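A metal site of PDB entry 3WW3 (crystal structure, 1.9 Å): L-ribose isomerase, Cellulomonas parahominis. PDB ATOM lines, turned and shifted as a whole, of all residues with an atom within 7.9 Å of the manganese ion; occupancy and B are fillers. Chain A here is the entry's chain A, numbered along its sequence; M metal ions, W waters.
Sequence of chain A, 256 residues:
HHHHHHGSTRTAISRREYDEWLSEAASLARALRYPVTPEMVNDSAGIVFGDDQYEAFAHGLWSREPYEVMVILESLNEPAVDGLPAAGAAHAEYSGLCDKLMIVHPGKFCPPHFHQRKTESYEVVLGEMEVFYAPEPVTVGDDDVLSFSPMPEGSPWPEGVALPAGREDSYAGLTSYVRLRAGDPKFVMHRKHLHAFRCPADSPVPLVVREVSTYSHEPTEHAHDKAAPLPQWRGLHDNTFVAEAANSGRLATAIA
OE1 of Glu 120 lies within hydrogen-bond range of OH of Tyr 122 (2.7 Å). ND1 of His 115 is in hydrogen-bond range of OD1 of Asn 239 (2.7 Å). O of Pro 111 lies within hydrogen-bond range of ND1 of His 113. The backbone carbonyl oxygen (O) of Glu 120 sits at hydrogen-bond distance from the backbone NH (N) of Met 189. O of His 193 is in hydrogen-bond range of ND1 of His 195, 2.8 Å away. A ring nitrogen (ND1) of His 115 lies within hydrogen-bond range of the backbone carbonyl oxygen (O) of Asp 238 (2.8 Å). The side-chain carboxylate (OE2) of Glu 120 sits close to the side-chain amino group (NZ) of Lys 118, at 3.2 Å.
The manganese ion is bound by a ring nitrogen (NE2) of His 115 (2.2 Å). Water W1 binds the manganese ion, 2.2 Å away. The manganese ion is bound by NE2 of His 113 (2.2 Å). Water W2 binds the manganese ion (2.3 Å). OE2 of Glu 120 binds the manganese ion (2.3 Å). NE2 of His 195 binds the manganese ion, 2.3 Å away.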
ATOM      1  N   LYS A 100      -5.246 -15.274 -25.176  1.00  0.00           N
ATOM      2  CA  LYS A 100      -6.522 -15.915 -24.897  1.00  0.00           C
ATOM      3  C   LYS A 100      -6.985 -16.698 -26.111  1.00  0.00           C
ATOM      4  O   LYS A 100      -6.626 -16.369 -27.257  1.00  0.00           O
ATOM      5  CB  LYS A 100      -7.572 -14.859 -24.537  1.00  0.00           C
ATOM      6  CG  LYS A 100      -8.086 -14.059 -25.721  1.00  0.00           C
ATOM      7  CD  LYS A 100      -8.522 -12.654 -25.328  1.00  0.00           C
ATOM      8  CE  LYS A 100      -7.314 -11.716 -25.199  1.00  0.00           C
ATOM      9  NZ  LYS A 100      -7.689 -10.273 -25.064  1.00  0.00           N
ATOM     10  N   MET A 102     -10.354 -17.956 -28.064  1.00  0.00           N
ATOM     11  CA  MET A 102     -11.771 -17.659 -28.175  1.00  0.00           C
ATOM     12  C   MET A 102     -12.460 -18.768 -28.983  1.00  0.00           C
ATOM     13  O   MET A 102     -11.963 -19.192 -30.031  1.00  0.00           O
ATOM     14  CB  MET A 102     -11.956 -16.296 -28.867  1.00  0.00           C
ATOM     15  CG  MET A 102     -11.099 -15.176 -28.254  1.00  0.00           C
ATOM     16  SD  MET A 102     -11.342 -13.541 -29.004  1.00  0.00           S
ATOM     17  CE  MET A 102     -10.461 -13.701 -30.541  1.00  0.00           C
ATOM     18  N   CYS A 110     -19.033 -12.096 -31.632  1.00  0.00           N
ATOM     19  CA  CYS A 110     -18.345 -11.378 -30.562  1.00  0.00           C
ATOM     20  C   CYS A 110     -18.880 -10.049 -31.100  1.00  0.00           C
ATOM     21  O   CYS A 110     -18.536  -9.640 -32.210  1.00  0.00           O
ATOM     22  CB  CYS A 110     -16.831 -11.421 -30.699  1.00  0.00           C
ATOM     23  SG  CYS A 110     -16.000 -10.286 -29.539  1.00  0.00           S
ATOM     24  N   PRO A 111     -19.752  -9.368 -30.346  1.00  0.00           N
ATOM     25  CA  PRO A 111     -20.370  -8.088 -30.723  1.00  0.00           C
ATOM     26  C   PRO A 111     -19.506  -6.858 -30.967  1.00  0.00           C
ATOM     27  O   PRO A 111     -18.375  -6.750 -30.484  1.00  0.00           O
ATOM     28  CB  PRO A 111     -21.378  -7.867 -29.603  1.00  0.00           C
ATOM     29  CG  PRO A 111     -20.638  -8.365 -28.427  1.00  0.00           C
ATOM     30  CD  PRO A 111     -20.022  -9.662 -28.927  1.00  0.00           C
ATOM     31  N   PRO A 112     -20.051  -5.878 -31.721  1.00  0.00           N
ATOM     32  CA  PRO A 112     -19.399  -4.610 -32.063  1.00  0.00           C
ATOM     33  C   PRO A 112     -18.942  -3.863 -30.804  1.00  0.00           C
ATOM     34  O   PRO A 112     -19.744  -3.615 -29.898  1.00  0.00           O
ATOM     35  CB  PRO A 112     -20.491  -3.857 -32.819  1.00  0.00           C
ATOM     36  CG  PRO A 112     -21.222  -4.959 -33.517  1.00  0.00           C
ATOM     37  CD  PRO A 112     -21.347  -5.993 -32.416  1.00  0.00           C
ATOM     38  N   HIS A 113     -17.663  -3.510 -30.773  1.00  0.00           N
ATOM     39  CA  HIS A 113     -17.096  -2.787 -29.643  1.00  0.00           C
ATOM     40  C   HIS A 113     -15.717  -2.267 -30.007  1.00  0.00           C
ATOM     41  O   HIS A 113     -15.178  -2.619 -31.066  1.00  0.00           O
ATOM     42  CB  HIS A 113     -16.947  -3.718 -28.438  1.00  0.00           C
ATOM     43  CG  HIS A 113     -15.900  -4.776 -28.628  1.00  0.00           C
ATOM     44  ND1 HIS A 113     -16.101  -5.878 -29.425  1.00  0.00           N
ATOM     45  CD2 HIS A 113     -14.639  -4.876 -28.158  1.00  0.00           C
ATOM     46  CE1 HIS A 113     -14.998  -6.610 -29.436  1.00  0.00           C
ATOM     47  NE2 HIS A 113     -14.096  -6.016 -28.674  1.00  0.00           N
ATOM     48  N   PHE A 114     -15.152  -1.437 -29.142  1.00  0.00           N
ATOM     49  CA  PHE A 114     -13.803  -0.936 -29.366  1.00  0.00           C
ATOM     50  C   PHE A 114     -13.109  -0.813 -28.009  1.00  0.00           C
ATOM     51  O   PHE A 114     -13.773  -0.804 -26.973  1.00  0.00           O
ATOM     52  CB  PHE A 114     -13.816   0.411 -30.105  1.00  0.00           C
ATOM     53  CG  PHE A 114     -14.240   1.587 -29.259  1.00  0.00           C
ATOM     54  CD1 PHE A 114     -13.370   2.137 -28.320  1.00  0.00           C
ATOM     55  CD2 PHE A 114     -15.482   2.179 -29.451  1.00  0.00           C
ATOM     56  CE1 PHE A 114     -13.733   3.268 -27.592  1.00  0.00           C
ATOM     57  CE2 PHE A 114     -15.859   3.310 -28.718  1.00  0.00           C
ATOM     58  CZ  PHE A 114     -14.986   3.856 -27.793  1.00  0.00           C
ATOM     59  N   HIS A 115     -11.794  -0.760 -28.035  1.00  0.00           N
ATOM     60  CA  HIS A 115     -10.995  -0.628 -26.817  1.00  0.00           C
ATOM     61  C   HIS A 115     -10.186   0.640 -26.947  1.00  0.00           C
ATOM     62  O   HIS A 115      -9.627   0.915 -28.007  1.00  0.00           O
ATOM     63  CB  HIS A 115     -10.024  -1.805 -26.649  1.00  0.00           C
ATOM     64  CG  HIS A 115     -10.667  -3.140 -26.776  1.00  0.00           C
ATOM     65  ND1 HIS A 115     -11.507  -3.661 -25.814  1.00  0.00           N
ATOM     66  CD2 HIS A 115     -10.603  -4.068 -27.757  1.00  0.00           C
ATOM     67  CE1 HIS A 115     -11.935  -4.845 -26.193  1.00  0.00           C
ATOM     68  NE2 HIS A 115     -11.403  -5.120 -27.369  1.00  0.00           N
ATOM     69  N   LYS A 118      -6.433  -1.367 -25.639  1.00  0.00           N
ATOM     70  CA  LYS A 118      -6.009  -2.647 -26.185  1.00  0.00           C
ATOM     71  C   LYS A 118      -5.955  -2.839 -27.703  1.00  0.00           C
ATOM     72  O   LYS A 118      -6.936  -2.616 -28.414  1.00  0.00           O
ATOM     73  CB  LYS A 118      -6.873  -3.764 -25.570  1.00  0.00           C
ATOM     74  CG  LYS A 118      -6.381  -5.170 -25.894  1.00  0.00           C
ATOM     75  CD  LYS A 118      -7.273  -6.257 -25.292  1.00  0.00           C
ATOM     76  CE  LYS A 118      -8.653  -6.257 -25.913  1.00  0.00           C
ATOM     77  NZ  LYS A 118      -9.473  -7.419 -25.457  1.00  0.00           N
ATOM     78  N   THR A 119      -4.778  -3.260 -28.181  1.00  0.00           N
ATOM     79  CA  THR A 119      -4.571  -3.559 -29.593  1.00  0.00           C
ATOM     80  C   THR A 119      -4.516  -5.086 -29.615  1.00  0.00           C
ATOM     81  O   THR A 119      -3.856  -5.693 -28.766  1.00  0.00           O
ATOM     82  CB  THR A 119      -3.233  -2.970 -30.107  1.00  0.00           C
ATOM     83  OG1 THR A 119      -3.391  -1.564 -30.295  1.00  0.00           O
ATOM     84  CG2 THR A 119      -2.839  -3.626 -31.440  1.00  0.00           C
ATOM     85  N   GLU A 120      -5.210  -5.699 -30.565  1.00  0.00           N
ATOM     86  CA  GLU A 120      -5.264  -7.153 -30.654  1.00  0.00           C
ATOM     87  C   GLU A 120      -4.727  -7.713 -31.972  1.00  0.00           C
ATOM     88  O   GLU A 120      -4.487  -6.982 -32.923  1.00  0.00           O
ATOM     89  CB  GLU A 120      -6.717  -7.648 -30.503  1.00  0.00           C
ATOM     90  CG  GLU A 120      -7.643  -6.710 -29.758  1.00  0.00           C
ATOM     91  CD  GLU A 120      -9.091  -7.202 -29.732  1.00  0.00           C
ATOM     92  OE1 GLU A 120      -9.617  -7.574 -30.803  1.00  0.00           O
ATOM     93  OE2 GLU A 120      -9.690  -7.203 -28.645  1.00  0.00           O
ATOM     94  N   TYR A 122      -5.164 -11.553 -34.376  1.00  0.00           N
ATOM     95  CA  TYR A 122      -5.882 -12.817 -34.483  1.00  0.00           C
ATOM     96  C   TYR A 122      -5.148 -13.901 -35.254  1.00  0.00           C
ATOM     97  O   TYR A 122      -4.548 -13.642 -36.303  1.00  0.00           O
ATOM     98  CB  TYR A 122      -7.246 -12.628 -35.164  1.00  0.00           C
ATOM     99  CG  TYR A 122      -8.044 -11.457 -34.664  1.00  0.00           C
ATOM    100  CD1 TYR A 122      -8.225 -11.235 -33.302  1.00  0.00           C
ATOM    101  CD2 TYR A 122      -8.622 -10.567 -35.564  1.00  0.00           C
ATOM    102  CE1 TYR A 122      -8.968 -10.144 -32.853  1.00  0.00           C
ATOM    103  CE2 TYR A 122      -9.362  -9.480 -35.128  1.00  0.00           C
ATOM    104  CZ  TYR A 122      -9.529  -9.275 -33.766  1.00  0.00           C
ATOM    105  OH  TYR A 122     -10.246  -8.184 -33.327  1.00  0.00           O
ATOM    106  N   MET A 189      -5.717  -5.776 -35.099  1.00  0.00           N
ATOM    107  CA  MET A 189      -6.844  -4.868 -34.879  1.00  0.00           C
ATOM    108  C   MET A 189      -6.365  -3.813 -33.887  1.00  0.00           C
ATOM    109  O   MET A 189      -6.344  -4.040 -32.677  1.00  0.00           O
ATOM    110  CB  MET A 189      -8.043  -5.623 -34.297  1.00  0.00           C
ATOM    111  CG  MET A 189      -9.296  -4.755 -34.088  1.00  0.00           C
ATOM    112  SD  MET A 189      -9.898  -4.010 -35.621  1.00  0.00           S
ATOM    113  CE  MET A 189     -10.407  -5.465 -36.524  1.00  0.00           C
ATOM    114  N   HIS A 193     -10.551   0.901 -32.564  1.00  0.00           N
ATOM    115  CA  HIS A 193     -11.196   0.518 -33.809  1.00  0.00           C
ATOM    116  C   HIS A 193     -12.393  -0.346 -33.496  1.00  0.00           C
ATOM    117  O   HIS A 193     -12.281  -1.321 -32.746  1.00  0.00           O
ATOM    118  CB  HIS A 193     -10.225  -0.238 -34.719  1.00  0.00           C
ATOM    119  CG  HIS A 193      -9.296   0.648 -35.477  1.00  0.00           C
ATOM    120  ND1 HIS A 193      -9.597   1.143 -36.730  1.00  0.00           N
ATOM    121  CD2 HIS A 193      -8.093   1.164 -35.153  1.00  0.00           C
ATOM    122  CE1 HIS A 193      -8.618   1.931 -37.137  1.00  0.00           C
ATOM    123  NE2 HIS A 193      -7.690   1.963 -36.197  1.00  0.00           N
ATOM    124  N   LEU A 194     -13.548   0.022 -34.031  1.00  0.00           N
ATOM    125  CA  LEU A 194     -14.746  -0.756 -33.821  1.00  0.00           C
ATOM    126  C   LEU A 194     -14.574  -2.080 -34.548  1.00  0.00           C
ATOM    127  O   LEU A 194     -14.155  -2.104 -35.711  1.00  0.00           O
ATOM    128  CB  LEU A 194     -15.968  -0.027 -34.400  1.00  0.00           C
ATOM    129  CG  LEU A 194     -16.571   1.122 -33.586  1.00  0.00           C
ATOM    130  CD1 LEU A 194     -17.671   1.775 -34.398  1.00  0.00           C
ATOM    131  CD2 LEU A 194     -17.126   0.586 -32.273  1.00  0.00           C
ATOM    132  N   HIS A 195     -14.868  -3.173 -33.868  1.00  0.00           N
ATOM    133  CA  HIS A 195     -14.740  -4.485 -34.495  1.00  0.00           C
ATOM    134  C   HIS A 195     -15.693  -5.505 -33.913  1.00  0.00           C
ATOM    135  O   HIS A 195     -16.255  -5.307 -32.834  1.00  0.00           O
ATOM    136  CB  HIS A 195     -13.306  -5.012 -34.374  1.00  0.00           C
ATOM    137  CG  HIS A 195     -12.807  -5.134 -32.967  1.00  0.00           C
ATOM    138  ND1 HIS A 195     -12.478  -4.043 -32.188  1.00  0.00           N
ATOM    139  CD2 HIS A 195     -12.567  -6.222 -32.194  1.00  0.00           C
ATOM    140  CE1 HIS A 195     -12.066  -4.455 -31.003  1.00  0.00           C
ATOM    141  NE2 HIS A 195     -12.106  -5.768 -30.978  1.00  0.00           N
ATOM    142  N   ALA A 196     -15.875  -6.593 -34.645  1.00  0.00           N
ATOM    143  CA  ALA A 196     -16.754  -7.692 -34.245  1.00  0.00           C
ATOM    144  C   ALA A 196     -16.382  -8.858 -35.147  1.00  0.00           C
ATOM    145  O   ALA A 196     -15.687  -8.673 -36.145  1.00  0.00           O
ATOM    146  CB  ALA A 196     -18.217  -7.319 -34.457  1.00  0.00           C
ATOM    147  N   PHE A 197     -16.811 -10.060 -34.797  1.00  0.00           N
ATOM    148  CA  PHE A 197     -16.528 -11.198 -35.656  1.00  0.00           C
ATOM    149  C   PHE A 197     -17.486 -12.334 -35.364  1.00  0.00           C
ATOM    150  O   PHE A 197     -18.128 -12.379 -34.310  1.00  0.00           O
ATOM    151  CB  PHE A 197     -15.063 -11.652 -35.496  1.00  0.00           C
ATOM    152  CG  PHE A 197     -14.759 -12.360 -34.210  1.00  0.00           C
ATOM    153  CD1 PHE A 197     -14.921 -13.741 -34.107  1.00  0.00           C
ATOM    154  CD2 PHE A 197     -14.258 -11.670 -33.113  1.00  0.00           C
ATOM    155  CE1 PHE A 197     -14.598 -14.417 -32.930  1.00  0.00           C
ATOM    156  CE2 PHE A 197     -13.923 -12.330 -31.923  1.00  0.00           C
ATOM    157  CZ  PHE A 197     -14.099 -13.711 -31.838  1.00  0.00           C
ATOM    158  N   GLU A 211      -5.958 -15.111 -29.579  1.00  0.00           N
ATOM    159  CA  GLU A 211      -5.786 -13.676 -29.597  1.00  0.00           C
ATOM    160  C   GLU A 211      -4.615 -13.289 -28.720  1.00  0.00           C
ATOM    161  O   GLU A 211      -4.543 -13.666 -27.551  1.00  0.00           O
ATOM    162  CB  GLU A 211      -7.041 -12.955 -29.114  1.00  0.00           C
ATOM    163  CG  GLU A 211      -6.894 -11.446 -29.119  1.00  0.00           C
ATOM    164  CD  GLU A 211      -8.168 -10.726 -28.765  1.00  0.00           C
ATOM    165  OE1 GLU A 211      -9.145 -10.843 -29.536  1.00  0.00           O
ATOM    166  OE2 GLU A 211      -8.204 -10.038 -27.725  1.00  0.00           O
ATOM    167  N   SER A 213      -2.803  -9.922 -27.499  1.00  0.00           N
ATOM    168  CA  SER A 213      -3.061  -8.480 -27.454  1.00  0.00           C
ATOM    169  C   SER A 213      -2.338  -7.842 -26.290  1.00  0.00           C
ATOM    170  O   SER A 213      -1.630  -8.510 -25.550  1.00  0.00           O
ATOM    171  CB  SER A 213      -4.561  -8.254 -27.265  1.00  0.00           C
ATOM    172  OG  SER A 213      -4.978  -8.661 -25.968  1.00  0.00           O
ATOM    173  N   ASP A 238     -12.078  -0.817 -20.296  1.00  0.00           N
ATOM    174  CA  ASP A 238     -11.485  -0.671 -21.621  1.00  0.00           C
ATOM    175  C   ASP A 238     -12.253  -1.376 -22.724  1.00  0.00           C
ATOM    176  O   ASP A 238     -11.680  -1.733 -23.753  1.00  0.00           O
ATOM    177  CB  ASP A 238     -10.037  -1.172 -21.586  1.00  0.00           C
ATOM    178  CG  ASP A 238      -9.241  -0.736 -22.801  1.00  0.00           C
ATOM    179  OD1 ASP A 238      -9.224   0.482 -23.079  1.00  0.00           O
ATOM    180  OD2 ASP A 238      -8.632  -1.598 -23.465  1.00  0.00           O
ATOM    181  N   ASN A 239     -13.549  -1.590 -22.505  1.00  0.00           N
ATOM    182  CA  ASN A 239     -14.394  -2.247 -23.493  1.00  0.00           C
ATOM    183  C   ASN A 239     -15.655  -1.421 -23.682  1.00  0.00           C
ATOM    184  O   ASN A 239     -16.459  -1.306 -22.757  1.00  0.00           O
ATOM    185  CB  ASN A 239     -14.779  -3.658 -23.044  1.00  0.00           C
ATOM    186  CG  ASN A 239     -13.597  -4.614 -22.999  1.00  0.00           C
ATOM    187  OD1 ASN A 239     -12.467  -4.233 -23.319  1.00  0.00           O
ATOM    188  ND2 ASN A 239     -13.857  -5.853 -22.602  1.00  0.00           N
ATOM    189  N   PHE A 241     -18.998  -1.184 -25.938  1.00  0.00           N
ATOM    190  CA  PHE A 241     -19.848  -1.834 -26.922  1.00  0.00           C
ATOM    191  C   PHE A 241     -20.818  -0.850 -27.559  1.00  0.00           C
ATOM    192  O   PHE A 241     -21.256   0.104 -26.925  1.00  0.00           O
ATOM    193  CB  PHE A 241     -20.637  -2.974 -26.266  1.00  0.00           C
ATOM    194  CG  PHE A 241     -19.762  -4.068 -25.735  1.00  0.00           C
ATOM    195  CD1 PHE A 241     -19.078  -3.913 -24.522  1.00  0.00           C
ATOM    196  CD2 PHE A 241     -19.568  -5.235 -26.469  1.00  0.00           C
ATOM    197  CE1 PHE A 241     -18.221  -4.900 -24.059  1.00  0.00           C
ATOM    198  CE2 PHE A 241     -18.711  -6.223 -26.006  1.00  0.00           C
ATOM    199  CZ  PHE A 241     -18.040  -6.067 -24.810  1.00  0.00           C
ATOM    200  N   ARG A 250     -21.598  -8.575 -19.820  1.00  0.00           N
ATOM    201  CA  ARG A 250     -20.151  -8.657 -19.855  1.00  0.00           C
ATOM    202  C   ARG A 250     -19.668  -8.608 -18.413  1.00  0.00           C
ATOM    203  O   ARG A 250     -18.527  -8.959 -18.115  1.00  0.00           O
ATOM    204  CB  ARG A 250     -19.582  -7.456 -20.632  1.00  0.00           C
ATOM    205  CG  ARG A 250     -18.066  -7.408 -20.725  1.00  0.00           C
ATOM    206  CD  ARG A 250     -17.512  -8.479 -21.649  1.00  0.00           C
ATOM    207  NE  ARG A 250     -16.067  -8.355 -21.834  1.00  0.00           N
ATOM    208  CZ  ARG A 250     -15.337  -9.105 -22.638  1.00  0.00           C
ATOM    209  NH1 ARG A 250     -15.917 -10.061 -23.363  1.00  0.00           N
ATOM    210  NH2 ARG A 250     -14.025  -8.916 -22.737  1.00  0.00           N
HETATM  211 MN    MN M   1     -11.938  -6.636 -28.816  1.00  0.00          MN
HETATM  212  O   HOH W   1     -11.925  -7.968 -27.029  1.00  0.00           O
HETATM  213  O   HOH W   2     -12.270  -8.629 -29.839  1.00  0.00           O
